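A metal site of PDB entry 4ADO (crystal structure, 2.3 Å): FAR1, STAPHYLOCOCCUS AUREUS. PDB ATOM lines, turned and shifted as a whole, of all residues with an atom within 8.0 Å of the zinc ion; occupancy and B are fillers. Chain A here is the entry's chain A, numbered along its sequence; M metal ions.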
ATOM      1  N   PHE A 128       2.401  10.886 -19.168  1.00  0.00           N
ATOM      2  CA  PHE A 128       2.314  10.547 -17.768  1.00  0.00           C
ATOM      3  C   PHE A 128       3.574   9.784 -17.402  1.00  0.00           C
ATOM      4  O   PHE A 128       4.295   9.369 -18.301  1.00  0.00           O
ATOM      5  CB  PHE A 128       1.067   9.719 -17.452  1.00  0.00           C
ATOM      6  CG  PHE A 128       1.130   8.331 -17.983  1.00  0.00           C
ATOM      7  CD1 PHE A 128       0.782   8.057 -19.300  1.00  0.00           C
ATOM      8  CD2 PHE A 128       1.573   7.299 -17.163  1.00  0.00           C
ATOM      9  CE1 PHE A 128       0.859   6.729 -19.779  1.00  0.00           C
ATOM     10  CE2 PHE A 128       1.661   6.005 -17.640  1.00  0.00           C
ATOM     11  CZ  PHE A 128       1.283   5.723 -18.953  1.00  0.00           C
ATOM     12  N   GLY A 164      -1.815  -8.141 -25.705  1.00  0.00           N
ATOM     13  CA  GLY A 164      -3.116  -7.559 -25.823  1.00  0.00           C
ATOM     14  C   GLY A 164      -3.076  -6.073 -26.047  1.00  0.00           C
ATOM     15  O   GLY A 164      -2.022  -5.431 -25.846  1.00  0.00           O
ATOM     16  N   PHE A 165      -4.241  -5.490 -26.274  1.00  0.00           N
ATOM     17  CA  PHE A 165      -4.298  -4.046 -26.465  1.00  0.00           C
ATOM     18  C   PHE A 165      -4.289  -3.300 -25.156  1.00  0.00           C
ATOM     19  O   PHE A 165      -5.058  -3.594 -24.291  1.00  0.00           O
ATOM     20  CB  PHE A 165      -5.545  -3.616 -27.265  1.00  0.00           C
ATOM     21  CG  PHE A 165      -5.483  -3.935 -28.711  1.00  0.00           C
ATOM     22  CD1 PHE A 165      -5.716  -5.223 -29.174  1.00  0.00           C
ATOM     23  CD2 PHE A 165      -5.066  -2.954 -29.619  1.00  0.00           C
ATOM     24  CE1 PHE A 165      -5.618  -5.530 -30.509  1.00  0.00           C
ATOM     25  CE2 PHE A 165      -4.963  -3.241 -30.976  1.00  0.00           C
ATOM     26  CZ  PHE A 165      -5.236  -4.555 -31.422  1.00  0.00           C
ATOM     27  N   CYS A 166      -3.343  -2.378 -25.018  1.00  0.00           N
ATOM     28  CA  CYS A 166      -3.265  -1.570 -23.813  1.00  0.00           C
ATOM     29  C   CYS A 166      -4.499  -0.633 -23.734  1.00  0.00           C
ATOM     30  O   CYS A 166      -4.898  -0.054 -24.743  1.00  0.00           O
ATOM     31  CB  CYS A 166      -1.979  -0.760 -23.806  1.00  0.00           C
ATOM     32  SG  CYS A 166      -1.950   0.409 -22.398  1.00  0.00           S
ATOM     33  N   THR A 167      -5.135  -0.553 -22.564  1.00  0.00           N
ATOM     34  CA  THR A 167      -6.295   0.344 -22.383  1.00  0.00           C
ATOM     35  C   THR A 167      -5.951   1.836 -22.446  1.00  0.00           C
ATOM     36  O   THR A 167      -6.804   2.674 -22.726  1.00  0.00           O
ATOM     37  CB  THR A 167      -7.031   0.093 -21.061  1.00  0.00           C
ATOM     38  OG1 THR A 167      -7.495  -1.266 -21.053  1.00  0.00           O
ATOM     39  CG2 THR A 167      -8.249   0.998 -20.975  1.00  0.00           C
ATOM     40  N   ILE A 168      -4.698   2.169 -22.135  1.00  0.00           N
ATOM     41  CA  ILE A 168      -4.209   3.544 -22.177  1.00  0.00           C
ATOM     42  C   ILE A 168      -3.820   4.011 -23.550  1.00  0.00           C
ATOM     43  O   ILE A 168      -4.349   5.015 -24.027  1.00  0.00           O
ATOM     44  CB  ILE A 168      -3.031   3.754 -21.272  1.00  0.00           C
ATOM     45  CG1 ILE A 168      -3.429   3.643 -19.812  1.00  0.00           C
ATOM     46  CG2 ILE A 168      -2.413   5.134 -21.534  1.00  0.00           C
ATOM     47  CD1 ILE A 168      -2.209   3.615 -18.880  1.00  0.00           C
ATOM     48  N   CYS A 169      -2.885   3.282 -24.162  1.00  0.00           N
ATOM     49  CA  CYS A 169      -2.329   3.721 -25.447  1.00  0.00           C
ATOM     50  C   CYS A 169      -3.045   3.099 -26.630  1.00  0.00           C
ATOM     51  O   CYS A 169      -2.826   3.479 -27.790  1.00  0.00           O
ATOM     52  CB  CYS A 169      -0.839   3.459 -25.520  1.00  0.00           C
ATOM     53  SG  CYS A 169      -0.393   1.645 -25.558  1.00  0.00           S
ATOM     54  N   ASN A 170      -3.867   2.088 -26.345  1.00  0.00           N
ATOM     55  CA  ASN A 170      -4.653   1.455 -27.412  1.00  0.00           C
ATOM     56  C   ASN A 170      -3.787   0.665 -28.419  1.00  0.00           C
ATOM     57  O   ASN A 170      -4.186   0.494 -29.567  1.00  0.00           O
ATOM     58  CB  ASN A 170      -5.517   2.469 -28.180  1.00  0.00           C
ATOM     59  CG  ASN A 170      -6.673   1.816 -28.909  1.00  0.00           C
ATOM     60  OD1 ASN A 170      -7.259   0.825 -28.447  1.00  0.00           O
ATOM     61  ND2 ASN A 170      -6.953   2.325 -30.115  1.00  0.00           N
ATOM     62  N   LYS A 171      -2.584   0.288 -28.048  1.00  0.00           N
ATOM     63  CA  LYS A 171      -1.728  -0.541 -28.885  1.00  0.00           C
ATOM     64  C   LYS A 171      -1.561  -1.984 -28.381  1.00  0.00           C
ATOM     65  O   LYS A 171      -1.597  -2.247 -27.235  1.00  0.00           O
ATOM     66  CB  LYS A 171      -0.357   0.098 -29.080  1.00  0.00           C
ATOM     67  CG  LYS A 171      -0.294   0.971 -30.261  1.00  0.00           C
ATOM     68  CD  LYS A 171      -1.175   2.174 -29.964  1.00  0.00           C
ATOM     69  CE  LYS A 171      -1.193   3.175 -31.095  1.00  0.00           C
ATOM     70  NZ  LYS A 171      -1.157   4.597 -30.574  1.00  0.00           N
ATOM     71  N   GLU A 172      -1.375  -2.900 -29.301  1.00  0.00           N
ATOM     72  CA  GLU A 172      -1.169  -4.285 -28.944  1.00  0.00           C
ATOM     73  C   GLU A 172       0.233  -4.409 -28.345  1.00  0.00           C
ATOM     74  O   GLU A 172       1.228  -4.200 -29.016  1.00  0.00           O
ATOM     75  CB  GLU A 172      -1.311  -5.157 -30.187  1.00  0.00           C
ATOM     76  CG  GLU A 172      -1.703  -6.570 -29.916  1.00  0.00           C
ATOM     77  CD  GLU A 172      -0.472  -7.452 -29.656  1.00  0.00           C
ATOM     78  OE1 GLU A 172       0.630  -7.060 -30.075  1.00  0.00           O
ATOM     79  OE2 GLU A 172      -0.610  -8.574 -29.108  1.00  0.00           O
ATOM     80  N   SER A 173       0.317  -4.834 -27.093  1.00  0.00           N
ATOM     81  CA  SER A 173       1.553  -4.689 -26.341  1.00  0.00           C
ATOM     82  C   SER A 173       1.637  -5.781 -25.314  1.00  0.00           C
ATOM     83  O   SER A 173       0.771  -6.652 -25.239  1.00  0.00           O
ATOM     84  CB  SER A 173       1.594  -3.351 -25.574  1.00  0.00           C
ATOM     85  OG  SER A 173       1.240  -2.218 -26.351  1.00  0.00           O
ATOM     86  N   ASN A 174       2.715  -5.759 -24.549  1.00  0.00           N
ATOM     87  CA  ASN A 174       2.832  -6.594 -23.399  1.00  0.00           C
ATOM     88  C   ASN A 174       2.137  -5.887 -22.238  1.00  0.00           C
ATOM     89  O   ASN A 174       2.584  -4.864 -21.721  1.00  0.00           O
ATOM     90  CB  ASN A 174       4.301  -6.829 -23.095  1.00  0.00           C
ATOM     91  CG  ASN A 174       4.891  -7.876 -24.022  1.00  0.00           C
ATOM     92  OD1 ASN A 174       4.324  -8.159 -25.069  1.00  0.00           O
ATOM     93  ND2 ASN A 174       5.994  -8.493 -23.606  1.00  0.00           N
ATOM     94  N   VAL A 175       0.983  -6.423 -21.869  1.00  0.00           N
ATOM     95  CA  VAL A 175       0.114  -5.780 -20.907  1.00  0.00           C
ATOM     96  C   VAL A 175      -0.143  -6.625 -19.671  1.00  0.00           C
ATOM     97  O   VAL A 175       0.028  -7.846 -19.687  1.00  0.00           O
ATOM     98  CB  VAL A 175      -1.237  -5.372 -21.549  1.00  0.00           C
ATOM     99  CG1 VAL A 175      -1.037  -4.369 -22.683  1.00  0.00           C
ATOM    100  CG2 VAL A 175      -1.990  -6.607 -22.041  1.00  0.00           C
ATOM    101  N   TYR A 196      -6.341  -3.749 -18.259  1.00  0.00           N
ATOM    102  CA  TYR A 196      -5.011  -4.096 -18.743  1.00  0.00           C
ATOM    103  C   TYR A 196      -4.279  -2.922 -19.371  1.00  0.00           C
ATOM    104  O   TYR A 196      -4.801  -2.227 -20.227  1.00  0.00           O
ATOM    105  CB  TYR A 196      -5.126  -5.203 -19.787  1.00  0.00           C
ATOM    106  CG  TYR A 196      -5.482  -6.557 -19.290  1.00  0.00           C
ATOM    107  CD1 TYR A 196      -6.821  -6.928 -19.167  1.00  0.00           C
ATOM    108  CD2 TYR A 196      -4.507  -7.484 -18.993  1.00  0.00           C
ATOM    109  CE1 TYR A 196      -7.166  -8.189 -18.747  1.00  0.00           C
ATOM    110  CE2 TYR A 196      -4.835  -8.736 -18.557  1.00  0.00           C
ATOM    111  CZ  TYR A 196      -6.168  -9.094 -18.434  1.00  0.00           C
ATOM    112  OH  TYR A 196      -6.481 -10.354 -17.997  1.00  0.00           O
ATOM    113  N   ILE A 197      -3.044  -2.707 -18.916  1.00  0.00           N
ATOM    114  CA  ILE A 197      -2.208  -1.633 -19.473  1.00  0.00           C
ATOM    115  C   ILE A 197      -0.788  -2.130 -19.657  1.00  0.00           C
ATOM    116  O   ILE A 197      -0.409  -3.134 -19.051  1.00  0.00           O
ATOM    117  CB  ILE A 197      -2.201  -0.425 -18.533  1.00  0.00           C
ATOM    118  CG1 ILE A 197      -1.477  -0.750 -17.225  1.00  0.00           C
ATOM    119  CG2 ILE A 197      -3.658   0.094 -18.312  1.00  0.00           C
ATOM    120  CD1 ILE A 197      -1.376   0.447 -16.291  1.00  0.00           C
ATOM    121  N   CYS A 198      -0.006  -1.421 -20.467  1.00  0.00           N
ATOM    122  CA  CYS A 198       1.387  -1.801 -20.691  1.00  0.00           C
ATOM    123  C   CYS A 198       2.119  -1.960 -19.360  1.00  0.00           C
ATOM    124  O   CYS A 198       2.087  -1.122 -18.495  1.00  0.00           O
ATOM    125  CB  CYS A 198       2.110  -0.714 -21.508  1.00  0.00           C
ATOM    126  SG  CYS A 198       1.492  -0.648 -23.191  1.00  0.00           S
ATOM    127  N   ARG A 199       2.810  -3.064 -19.215  1.00  0.00           N
ATOM    128  CA  ARG A 199       3.643  -3.248 -18.061  1.00  0.00           C
ATOM    129  C   ARG A 199       4.735  -2.187 -18.052  1.00  0.00           C
ATOM    130  O   ARG A 199       5.039  -1.626 -17.029  1.00  0.00           O
ATOM    131  CB  ARG A 199       4.225  -4.654 -18.137  1.00  0.00           C
ATOM    132  CG  ARG A 199       4.947  -5.096 -16.925  1.00  0.00           C
ATOM    133  CD  ARG A 199       4.982  -6.605 -16.934  1.00  0.00           C
ATOM    134  NE  ARG A 199       5.391  -7.090 -15.630  1.00  0.00           N
ATOM    135  CZ  ARG A 199       4.506  -7.472 -14.734  1.00  0.00           C
ATOM    136  NH1 ARG A 199       3.226  -7.429 -15.058  1.00  0.00           N
ATOM    137  NH2 ARG A 199       4.881  -7.904 -13.539  1.00  0.00           N
ATOM    138  N   ASP A 200       5.289  -1.894 -19.230  1.00  0.00           N
ATOM    139  CA  ASP A 200       6.373  -0.892 -19.335  1.00  0.00           C
ATOM    140  C   ASP A 200       5.787   0.486 -19.741  1.00  0.00           C
ATOM    141  O   ASP A 200       5.457   0.687 -20.898  1.00  0.00           O
ATOM    142  CB  ASP A 200       7.362  -1.349 -20.391  1.00  0.00           C
ATOM    143  CG  ASP A 200       8.514  -0.376 -20.621  1.00  0.00           C
ATOM    144  OD1 ASP A 200       8.656   0.610 -19.864  1.00  0.00           O
ATOM    145  OD2 ASP A 200       9.280  -0.610 -21.583  1.00  0.00           O
ATOM    146  N   SER A 201       5.635   1.409 -18.791  1.00  0.00           N
ATOM    147  CA  SER A 201       4.948   2.680 -19.074  1.00  0.00           C
ATOM    148  C   SER A 201       5.698   3.659 -19.967  1.00  0.00           C
ATOM    149  O   SER A 201       5.082   4.482 -20.625  1.00  0.00           O
ATOM    150  CB  SER A 201       4.492   3.386 -17.798  1.00  0.00           C
ATOM    151  OG  SER A 201       3.414   2.697 -17.159  1.00  0.00           O
ATOM    152  N   ILE A 202       7.016   3.529 -20.056  1.00  0.00           N
ATOM    153  CA  ILE A 202       7.793   4.373 -20.948  1.00  0.00           C
ATOM    154  C   ILE A 202       7.445   4.068 -22.365  1.00  0.00           C
ATOM    155  O   ILE A 202       7.230   4.962 -23.179  1.00  0.00           O
ATOM    156  CB  ILE A 202       9.304   4.160 -20.685  1.00  0.00           C
ATOM    157  CG1 ILE A 202       9.641   4.710 -19.299  1.00  0.00           C
ATOM    158  CG2 ILE A 202      10.170   4.831 -21.771  1.00  0.00           C
ATOM    159  CD1 ILE A 202      11.039   4.388 -18.813  1.00  0.00           C
ATOM    160  N   HIS A 203       7.347   2.790 -22.655  1.00  0.00           N
ATOM    161  CA  HIS A 203       6.998   2.340 -23.964  1.00  0.00           C
ATOM    162  C   HIS A 203       5.541   2.699 -24.246  1.00  0.00           C
ATOM    163  O   HIS A 203       5.180   3.007 -25.385  1.00  0.00           O
ATOM    164  CB  HIS A 203       7.243   0.841 -24.063  1.00  0.00           C
ATOM    165  CG  HIS A 203       6.723   0.229 -25.317  1.00  0.00           C
ATOM    166  ND1 HIS A 203       7.316   0.451 -26.545  1.00  0.00           N
ATOM    167  CD2 HIS A 203       5.654  -0.568 -25.546  1.00  0.00           C
ATOM    168  CE1 HIS A 203       6.634  -0.198 -27.474  1.00  0.00           C
ATOM    169  NE2 HIS A 203       5.625  -0.831 -26.894  1.00  0.00           N
ATOM    170  N   CYS A 204       4.704   2.588 -23.232  1.00  0.00           N
ATOM    171  CA  CYS A 204       3.308   3.001 -23.291  1.00  0.00           C
ATOM    172  C   CYS A 204       3.198   4.496 -23.755  1.00  0.00           C
ATOM    173  O   CYS A 204       2.448   4.852 -24.670  1.00  0.00           O
ATOM    174  CB  CYS A 204       2.643   2.803 -21.925  1.00  0.00           C
ATOM    175  SG  CYS A 204       0.781   2.950 -21.895  1.00  0.00           S
ATOM    176  N   ASN A 205       3.935   5.364 -23.085  1.00  0.00           N
ATOM    177  CA  ASN A 205       3.910   6.774 -23.407  1.00  0.00           C
ATOM    178  C   ASN A 205       4.313   7.043 -24.856  1.00  0.00           C
ATOM    179  O   ASN A 205       3.679   7.867 -25.528  1.00  0.00           O
ATOM    180  CB  ASN A 205       4.776   7.545 -22.410  1.00  0.00           C
ATOM    181  CG  ASN A 205       3.994   7.917 -21.173  1.00  0.00           C
ATOM    182  OD1 ASN A 205       3.267   8.906 -21.162  1.00  0.00           O
ATOM    183  ND2 ASN A 205       4.072   7.088 -20.129  1.00  0.00           N
ATOM    184  N   LYS A 206       5.308   6.291 -25.332  1.00  0.00           N
ATOM    185  CA  LYS A 206       5.726   6.427 -26.728  1.00  0.00           C
ATOM    186  C   LYS A 206       4.640   6.039 -27.748  1.00  0.00           C
ATOM    187  O   LYS A 206       4.633   6.519 -28.865  1.00  0.00           O
ATOM    188  CB  LYS A 206       6.993   5.609 -27.042  1.00  0.00           C
ATOM    189  CG  LYS A 206       8.293   6.127 -26.458  1.00  0.00           C
ATOM    190  CD  LYS A 206       9.415   5.081 -26.664  1.00  0.00           C
ATOM    191  CE  LYS A 206      10.732   5.522 -26.003  1.00  0.00           C
ATOM    192  NZ  LYS A 206      10.513   6.483 -24.892  1.00  0.00           N
ATOM    193  N   GLN A 207       3.752   5.143 -27.365  1.00  0.00           N
ATOM    194  CA  GLN A 207       2.710   4.675 -28.253  1.00  0.00           C
ATOM    195  C   GLN A 207       1.448   5.494 -28.127  1.00  0.00           C
ATOM    196  O   GLN A 207       0.527   5.306 -28.911  1.00  0.00           O
ATOM    197  CB  GLN A 207       2.399   3.213 -27.945  1.00  0.00           C
ATOM    198  CG  GLN A 207       3.631   2.396 -28.158  1.00  0.00           C
ATOM    199  CD  GLN A 207       3.389   0.921 -27.961  1.00  0.00           C
ATOM    200  OE1 GLN A 207       3.007   0.480 -26.877  1.00  0.00           O
ATOM    201  NE2 GLN A 207       3.581   0.163 -29.022  1.00  0.00           N
ATOM    202  N   LEU A 208       1.429   6.410 -27.171  1.00  0.00           N
ATOM    203  CA  LEU A 208       0.226   7.155 -26.827  1.00  0.00           C
ATOM    204  C   LEU A 208       0.155   8.436 -27.677  1.00  0.00           C
ATOM    205  O   LEU A 208       0.888   9.395 -27.495  1.00  0.00           O
ATOM    206  CB  LEU A 208       0.226   7.452 -25.315  1.00  0.00           C
ATOM    207  CG  LEU A 208      -0.864   8.317 -24.657  1.00  0.00           C
ATOM    208  CD1 LEU A 208      -2.275   7.830 -24.928  1.00  0.00           C
ATOM    209  CD2 LEU A 208      -0.603   8.490 -23.130  1.00  0.00           C
HETATM  210 ZN    ZN M   1       0.120   1.286 -23.304  1.00  0.00          ZN
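Four residues have an atom within 4 Å of the zinc ion: Cys 166, Cys 169, Cys 198 and Cys 204.
O of Cys 169 lies close to NZ of Lys 171 (3.4 Å). The side-chain sulfur (SG) of Cys 198 lies close to the side-chain hydroxyl (OG) of Ser 173 (3.5 Å). The side-chain sulfur (SG) of Cys 166 lies close to the backbone NH (N) of Ile 168, at 3.3 Å. N of Cys 166 is in hydrogen-bond range of O of Lys 171, 2.8 Å away.
The zinc ion is bound by SG of Cys 204 (2.3 Å), SG of Cys 169 (2.3 Å), SG of Cys 198 (2.4 Å) and SG of Cys 166 (2.4 Å).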
